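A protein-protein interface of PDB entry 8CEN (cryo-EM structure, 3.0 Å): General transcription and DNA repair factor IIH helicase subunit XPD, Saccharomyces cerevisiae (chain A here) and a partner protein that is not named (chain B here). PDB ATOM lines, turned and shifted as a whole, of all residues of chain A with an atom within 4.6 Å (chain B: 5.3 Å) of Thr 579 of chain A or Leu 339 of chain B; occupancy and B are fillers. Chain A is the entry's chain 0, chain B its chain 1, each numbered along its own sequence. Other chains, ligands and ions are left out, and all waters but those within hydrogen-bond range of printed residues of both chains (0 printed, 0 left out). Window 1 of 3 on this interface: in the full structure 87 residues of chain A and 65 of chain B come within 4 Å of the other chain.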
ATOM      1  N   GLU A 572       1.534  29.311   5.459  1.00  0.00           N
ATOM      2  CA  GLU A 572       2.840  29.472   4.822  1.00  0.00           C
ATOM      3  C   GLU A 572       3.467  30.782   5.287  1.00  0.00           C
ATOM      4  O   GLU A 572       3.073  31.869   4.861  1.00  0.00           O
ATOM      5  CB  GLU A 572       2.698  29.428   3.305  1.00  0.00           C
ATOM      6  CG  GLU A 572       3.973  29.747   2.543  1.00  0.00           C
ATOM      7  CD  GLU A 572       3.736  29.920   1.057  1.00  0.00           C
ATOM      8  OE1 GLU A 572       2.564  30.057   0.654  1.00  0.00           O
ATOM      9  OE2 GLU A 572       4.722  29.918   0.290  1.00  0.00           O
ATOM     10  N   THR A 573       4.439  30.670   6.187  1.00  0.00           N
ATOM     11  CA  THR A 573       5.176  31.827   6.669  1.00  0.00           C
ATOM     12  C   THR A 573       6.124  32.319   5.573  1.00  0.00           C
ATOM     13  O   THR A 573       6.646  31.509   4.802  1.00  0.00           O
ATOM     14  CB  THR A 573       5.950  31.432   7.938  1.00  0.00           C
ATOM     15  OG1 THR A 573       5.023  30.974   8.930  1.00  0.00           O
ATOM     16  CG2 THR A 573       6.748  32.587   8.529  1.00  0.00           C
ATOM     17  N   PRO A 574       6.326  33.636   5.440  1.00  0.00           N
ATOM     18  CA  PRO A 574       7.370  34.121   4.519  1.00  0.00           C
ATOM     19  C   PRO A 574       8.768  33.644   4.879  1.00  0.00           C
ATOM     20  O   PRO A 574       9.613  33.508   3.986  1.00  0.00           O
ATOM     21  CB  PRO A 574       7.245  35.649   4.622  1.00  0.00           C
ATOM     22  CG  PRO A 574       6.475  35.894   5.884  1.00  0.00           C
ATOM     23  CD  PRO A 574       5.523  34.750   5.964  1.00  0.00           C
ATOM     24  N   ASP A 575       9.039  33.393   6.158  1.00  0.00           N
ATOM     25  CA  ASP A 575      10.297  32.774   6.547  1.00  0.00           C
ATOM     26  C   ASP A 575      10.299  31.308   6.132  1.00  0.00           C
ATOM     27  O   ASP A 575       9.364  30.560   6.441  1.00  0.00           O
ATOM     28  CB  ASP A 575      10.513  32.906   8.053  1.00  0.00           C
ATOM     29  CG  ASP A 575      11.886  32.430   8.490  1.00  0.00           C
ATOM     30  OD1 ASP A 575      12.812  32.420   7.651  1.00  0.00           O
ATOM     31  OD2 ASP A 575      12.039  32.068   9.675  1.00  0.00           O
ATOM     32  N   ALA A 576      11.363  30.895   5.439  1.00  0.00           N
ATOM     33  CA  ALA A 576      11.399  29.556   4.866  1.00  0.00           C
ATOM     34  C   ALA A 576      11.632  28.481   5.920  1.00  0.00           C
ATOM     35  O   ALA A 576      11.129  27.364   5.770  1.00  0.00           O
ATOM     36  CB  ALA A 576      12.467  29.481   3.783  1.00  0.00           C
ATOM     37  N   GLN A 577      12.389  28.794   6.979  1.00  0.00           N
ATOM     38  CA  GLN A 577      12.510  27.878   8.113  1.00  0.00           C
ATOM     39  C   GLN A 577      11.146  27.562   8.713  1.00  0.00           C
ATOM     40  O   GLN A 577      10.770  26.391   8.843  1.00  0.00           O
ATOM     41  CB  GLN A 577      13.426  28.475   9.185  1.00  0.00           C
ATOM     42  CG  GLN A 577      14.899  28.575   8.828  1.00  0.00           C
ATOM     43  CD  GLN A 577      15.557  27.213   8.676  1.00  0.00           C
ATOM     44  OE1 GLN A 577      15.771  26.504   9.657  1.00  0.00           O
ATOM     45  NE2 GLN A 577      15.885  26.848   7.451  1.00  0.00           N
ATOM     46  N   GLU A 578      10.379  28.600   9.049  1.00  0.00           N
ATOM     47  CA  GLU A 578       9.073  28.394   9.663  1.00  0.00           C
ATOM     48  C   GLU A 578       8.097  27.746   8.693  1.00  0.00           C
ATOM     49  O   GLU A 578       7.251  26.951   9.114  1.00  0.00           O
ATOM     50  CB  GLU A 578       8.521  29.721  10.175  1.00  0.00           C
ATOM     51  CG  GLU A 578       9.476  30.454  11.095  1.00  0.00           C
ATOM     52  CD  GLU A 578       8.833  31.636  11.773  1.00  0.00           C
ATOM     53  OE1 GLU A 578       7.600  31.789  11.655  1.00  0.00           O
ATOM     54  OE2 GLU A 578       9.560  32.416  12.422  1.00  0.00           O
ATOM     55  N   THR A 579       8.218  28.044   7.397  1.00  0.00           N
ATOM     56  CA  THR A 579       7.392  27.367   6.401  1.00  0.00           C
ATOM     57  C   THR A 579       7.720  25.877   6.325  1.00  0.00           C
ATOM     58  O   THR A 579       6.816  25.046   6.192  1.00  0.00           O
ATOM     59  CB  THR A 579       7.570  28.031   5.036  1.00  0.00           C
ATOM     60  OG1 THR A 579       7.391  29.443   5.171  1.00  0.00           O
ATOM     61  CG2 THR A 579       6.539  27.509   4.058  1.00  0.00           C
ATOM     62  N   SER A 580       9.006  25.518   6.420  1.00  0.00           N
ATOM     63  CA  SER A 580       9.398  24.111   6.367  1.00  0.00           C
ATOM     64  C   SER A 580       8.939  23.352   7.608  1.00  0.00           C
ATOM     65  O   SER A 580       8.474  22.209   7.504  1.00  0.00           O
ATOM     66  CB  SER A 580      10.913  23.999   6.199  1.00  0.00           C
ATOM     67  OG  SER A 580      11.324  24.498   4.938  1.00  0.00           O
ATOM     68  N   LEU A 581       9.067  23.965   8.791  1.00  0.00           N
ATOM     69  CA  LEU A 581       8.508  23.348   9.995  1.00  0.00           C
ATOM     70  C   LEU A 581       6.988  23.240   9.938  1.00  0.00           C
ATOM     71  O   LEU A 581       6.422  22.249  10.411  1.00  0.00           O
ATOM     72  CB  LEU A 581       8.943  24.092  11.260  1.00  0.00           C
ATOM     73  CG  LEU A 581      10.329  23.901  11.890  1.00  0.00           C
ATOM     74  CD1 LEU A 581      11.527  24.469  11.166  1.00  0.00           C
ATOM     75  CD2 LEU A 581      10.249  24.516  13.270  1.00  0.00           C
ATOM     76  N   ALA A 582       6.310  24.240   9.368  1.00  0.00           N
ATOM     77  CA  ALA A 582       4.863  24.145   9.205  1.00  0.00           C
ATOM     78  C   ALA A 582       4.489  23.014   8.255  1.00  0.00           C
ATOM     79  O   ALA A 582       3.526  22.282   8.498  1.00  0.00           O
ATOM     80  CB  ALA A 582       4.302  25.475   8.706  1.00  0.00           C
ATOM     81  N   LEU A 583       5.253  22.847   7.176  1.00  0.00           N
ATOM     82  CA  LEU A 583       4.997  21.762   6.234  1.00  0.00           C
ATOM     83  C   LEU A 583       5.238  20.397   6.872  1.00  0.00           C
ATOM     84  O   LEU A 583       4.461  19.458   6.655  1.00  0.00           O
ATOM     85  CB  LEU A 583       5.873  21.951   4.999  1.00  0.00           C
ATOM     86  CG  LEU A 583       5.810  20.935   3.867  1.00  0.00           C
ATOM     87  CD1 LEU A 583       4.378  20.731   3.400  1.00  0.00           C
ATOM     88  CD2 LEU A 583       6.685  21.447   2.742  1.00  0.00           C
ATOM     89  N   LYS A 605       6.317  29.658  -2.149  1.00  0.00           N
ATOM     90  CA  LYS A 605       7.344  28.622  -2.094  1.00  0.00           C
ATOM     91  C   LYS A 605       6.728  27.229  -2.058  1.00  0.00           C
ATOM     92  O   LYS A 605       7.273  26.288  -2.649  1.00  0.00           O
ATOM     93  CB  LYS A 605       8.236  28.840  -0.873  1.00  0.00           C
ATOM     94  CG  LYS A 605       8.667  30.281  -0.664  1.00  0.00           C
ATOM     95  CD  LYS A 605       9.377  30.449   0.669  1.00  0.00           C
ATOM     96  CE  LYS A 605       8.421  30.231   1.832  1.00  0.00           C
ATOM     97  NZ  LYS A 605       7.383  31.297   1.908  1.00  0.00           N
ATOM     98  N   VAL A 606       5.600  27.077  -1.360  1.00  0.00           N
ATOM     99  CA  VAL A 606       4.962  25.772  -1.211  1.00  0.00           C
ATOM    100  C   VAL A 606       4.401  25.282  -2.543  1.00  0.00           C
ATOM    101  O   VAL A 606       4.451  24.083  -2.843  1.00  0.00           O
ATOM    102  CB  VAL A 606       3.875  25.854  -0.122  1.00  0.00           C
ATOM    103  CG1 VAL A 606       3.167  24.523   0.055  1.00  0.00           C
ATOM    104  CG2 VAL A 606       4.482  26.307   1.191  1.00  0.00           C
ATOM    105  N   ILE A 610       6.866  21.243  -3.766  1.00  0.00           N
ATOM    106  CA  ILE A 610       6.260  20.454  -2.701  1.00  0.00           C
ATOM    107  C   ILE A 610       5.059  19.692  -3.241  1.00  0.00           C
ATOM    108  O   ILE A 610       4.173  20.268  -3.888  1.00  0.00           O
ATOM    109  CB  ILE A 610       5.862  21.357  -1.526  1.00  0.00           C
ATOM    110  CG1 ILE A 610       7.094  22.075  -0.965  1.00  0.00           C
ATOM    111  CG2 ILE A 610       5.152  20.551  -0.453  1.00  0.00           C
ATOM    112  CD1 ILE A 610       8.252  21.158  -0.633  1.00  0.00           C
ATOM    113  N   ILE B 337      11.479  18.540   1.834  1.00  0.00           N
ATOM    114  CA  ILE B 337      10.649  19.671   2.234  1.00  0.00           C
ATOM    115  C   ILE B 337      11.514  20.842   2.689  1.00  0.00           C
ATOM    116  O   ILE B 337      11.063  21.697   3.460  1.00  0.00           O
ATOM    117  CB  ILE B 337       9.663  19.255   3.340  1.00  0.00           C
ATOM    118  CG1 ILE B 337      10.413  18.638   4.519  1.00  0.00           C
ATOM    119  CG2 ILE B 337       8.631  18.274   2.801  1.00  0.00           C
ATOM    120  CD1 ILE B 337       9.640  18.667   5.811  1.00  0.00           C
ATOM    121  N   ASP B 338      12.757  20.898   2.210  1.00  0.00           N
ATOM    122  CA  ASP B 338      13.707  21.933   2.623  1.00  0.00           C
ATOM    123  C   ASP B 338      13.528  23.166   1.740  1.00  0.00           C
ATOM    124  O   ASP B 338      14.285  23.415   0.800  1.00  0.00           O
ATOM    125  CB  ASP B 338      15.135  21.406   2.556  1.00  0.00           C
ATOM    126  CG  ASP B 338      16.115  22.275   3.317  1.00  0.00           C
ATOM    127  OD1 ASP B 338      15.666  23.125   4.115  1.00  0.00           O
ATOM    128  OD2 ASP B 338      17.336  22.110   3.116  1.00  0.00           O
ATOM    129  N   LEU B 339      12.508  23.965   2.069  1.00  0.00           N
ATOM    130  CA  LEU B 339      12.223  25.172   1.298  1.00  0.00           C
ATOM    131  C   LEU B 339      13.287  26.248   1.478  1.00  0.00           C
ATOM    132  O   LEU B 339      13.481  27.072   0.574  1.00  0.00           O
ATOM    133  CB  LEU B 339      10.848  25.719   1.679  1.00  0.00           C
ATOM    134  CG  LEU B 339       9.678  24.986   1.021  1.00  0.00           C
ATOM    135  CD1 LEU B 339       8.380  25.276   1.745  1.00  0.00           C
ATOM    136  CD2 LEU B 339       9.570  25.373  -0.443  1.00  0.00           C
ATOM    137  N   ASP B 340      13.997  26.245   2.607  1.00  0.00           N
ATOM    138  CA  ASP B 340      15.107  27.176   2.773  1.00  0.00           C
ATOM    139  C   ASP B 340      16.243  26.818   1.823  1.00  0.00           C
ATOM    140  O   ASP B 340      16.836  27.701   1.197  1.00  0.00           O
ATOM    141  CB  ASP B 340      15.578  27.161   4.228  1.00  0.00           C
ATOM    142  CG  ASP B 340      16.591  28.263   4.551  1.00  0.00           C
ATOM    143  OD1 ASP B 340      16.979  29.051   3.664  1.00  0.00           O
ATOM    144  OD2 ASP B 340      17.006  28.339   5.727  1.00  0.00           O
ATOM    145  N   GLY B 341      16.545  25.526   1.688  1.00  0.00           N
ATOM    146  CA  GLY B 341      17.469  25.099   0.653  1.00  0.00           C
ATOM    147  C   GLY B 341      16.951  25.381  -0.742  1.00  0.00           C
ATOM    148  O   GLY B 341      17.730  25.687  -1.647  1.00  0.00           O
ATOM    149  N   ASN B 342      15.630  25.315  -0.925  1.00  0.00           N
ATOM    150  CA  ASN B 342      15.032  25.612  -2.222  1.00  0.00           C
ATOM    151  C   ASN B 342      15.250  27.068  -2.618  1.00  0.00           C
ATOM    152  O   ASN B 342      15.499  27.367  -3.791  1.00  0.00           O
ATOM    153  CB  ASN B 342      13.541  25.282  -2.195  1.00  0.00           C
ATOM    154  CG  ASN B 342      13.282  23.803  -2.042  1.00  0.00           C
ATOM    155  OD1 ASN B 342      14.167  22.981  -2.271  1.00  0.00           O
ATOM    156  ND2 ASN B 342      12.060  23.449  -1.664  1.00  0.00           N
ATOM    157  N   ILE B 343      15.167  27.989  -1.656  1.00  0.00           N
ATOM    158  CA  ILE B 343      15.391  29.395  -1.989  1.00  0.00           C
ATOM    159  C   ILE B 343      16.863  29.797  -1.925  1.00  0.00           C
ATOM    160  O   ILE B 343      17.243  30.804  -2.538  1.00  0.00           O
ATOM    161  CB  ILE B 343      14.581  30.353  -1.097  1.00  0.00           C
ATOM    162  CG1 ILE B 343      14.986  30.227   0.371  1.00  0.00           C
ATOM    163  CG2 ILE B 343      13.092  30.090  -1.258  1.00  0.00           C
ATOM    164  CD1 ILE B 343      14.395  31.305   1.246  1.00  0.00           C
ATOM    165  N   GLN B 344      17.700  29.048  -1.207  1.00  0.00           N
ATOM    166  CA  GLN B 344      19.133  29.310  -1.174  1.00  0.00           C
ATOM    167  C   GLN B 344      19.911  28.493  -2.195  1.00  0.00           C
ATOM    168  O   GLN B 344      21.145  28.529  -2.177  1.00  0.00           O
ATOM    169  CB  GLN B 344      19.697  29.050   0.228  1.00  0.00           C
ATOM    170  CG  GLN B 344      19.154  29.969   1.314  1.00  0.00           C
ATOM    171  CD  GLN B 344      19.555  31.421   1.119  1.00  0.00           C
ATOM    172  OE1 GLN B 344      20.574  31.722   0.498  1.00  0.00           O
ATOM    173  NE2 GLN B 344      18.746  32.331   1.649  1.00  0.00           N
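NE2 of Gln 577 of chain A sits at hydrogen-bond distance from OD2 of Asp 340 of chain B, 2.5 Å away.
The backbone carbonyl oxygen (O) of Ile 337 of chain B is in hydrogen-bond range of the side-chain hydroxyl (OG) of Ser 580 of chain A, at 3.2 Å.
The backbone NH of Leu 339 of chain B lies within hydrogen-bond range of the side-chain hydroxyl of Ser 580 of chain A (3.1 Å).
The side-chain carboxylate (OE2) of Glu 572 of chain A lies within salt-bridge range of the side-chain amino group (NZ) of Lys 605 of chain A, 3.4 Å away.
N of Thr 573 of chain A lies close to OG1 of Thr 579 of chain A (3.4 Å).
The side-chain amino group (NZ) of Lys 605 of chain A is in hydrogen-bond range of the backbone carbonyl oxygen (O) of Thr 573 of chain A, 3.0 Å away.
The backbone carbonyl oxygen of Asp 575 of chain A sits at hydrogen-bond distance from the side-chain hydroxyl of Thr 579 of chain A (2.6 Å).
The side-chain hydroxyl (OG) of Ser 580 of chain A sits at hydrogen-bond distance from the backbone carbonyl oxygen (O) of Ala 576 of chain A (3.0 Å).
Among the printed residues, pairs that only touch across the chains: Ala 576 of chain A with Asp 340 of chain B, Ala 576 of chain A with Ile 343 of chain B, Thr 579 of chain A with Leu 339 of chain B, Ser 580 of chain A with Asp 340 of chain B, Leu 583 of chain A with Ile 337 of chain B and Lys 605 of chain A with Leu 339 of chain B.
Thr 573 of chain A touches none of the printed residues of chain B.
Thr 579 of chain A touches one residue of chain B.
Of the printed residues of chain B, Ser 580 of chain A touches Ile 337, Leu 339 and Asp 340.
Leu 339 of chain B touches three residues of chain A.
Of the printed residues of chain A, Ile 343 of chain B touches Ala 576 (3.7 Å).
The nearest printed residue of chain B that does not touch Thr 579 of chain A is Ile 337 of chain B (6.1 Å).
The nearest printed residue of chain B that does not touch Ala 576 of chain A is Leu 339 of chain B (4.1 Å).
Of the 15 printed residues of chain A, 6 touch a printed residue of chain B.
Printed residues of chain A that touch a printed residue of chain B: Ala 576, Gln 577, Thr 579, Ser 580, Leu 583 and Lys 605.
Hydrophobic or aromatic side chains of chain A within 4 Å of the printed part of chain B: Ala 576 and Leu 583.
Printed residues of chain B that touch a printed residue of chain A: Ile 337, Leu 339, Asp 340 and Ile 343.
Hydrophobic or aromatic side chains of chain B within 4 Å of the printed part of chain A: Ile 337, Leu 339 and Ile 343.
Among the printed residues, 9 pairs touch across the chains.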
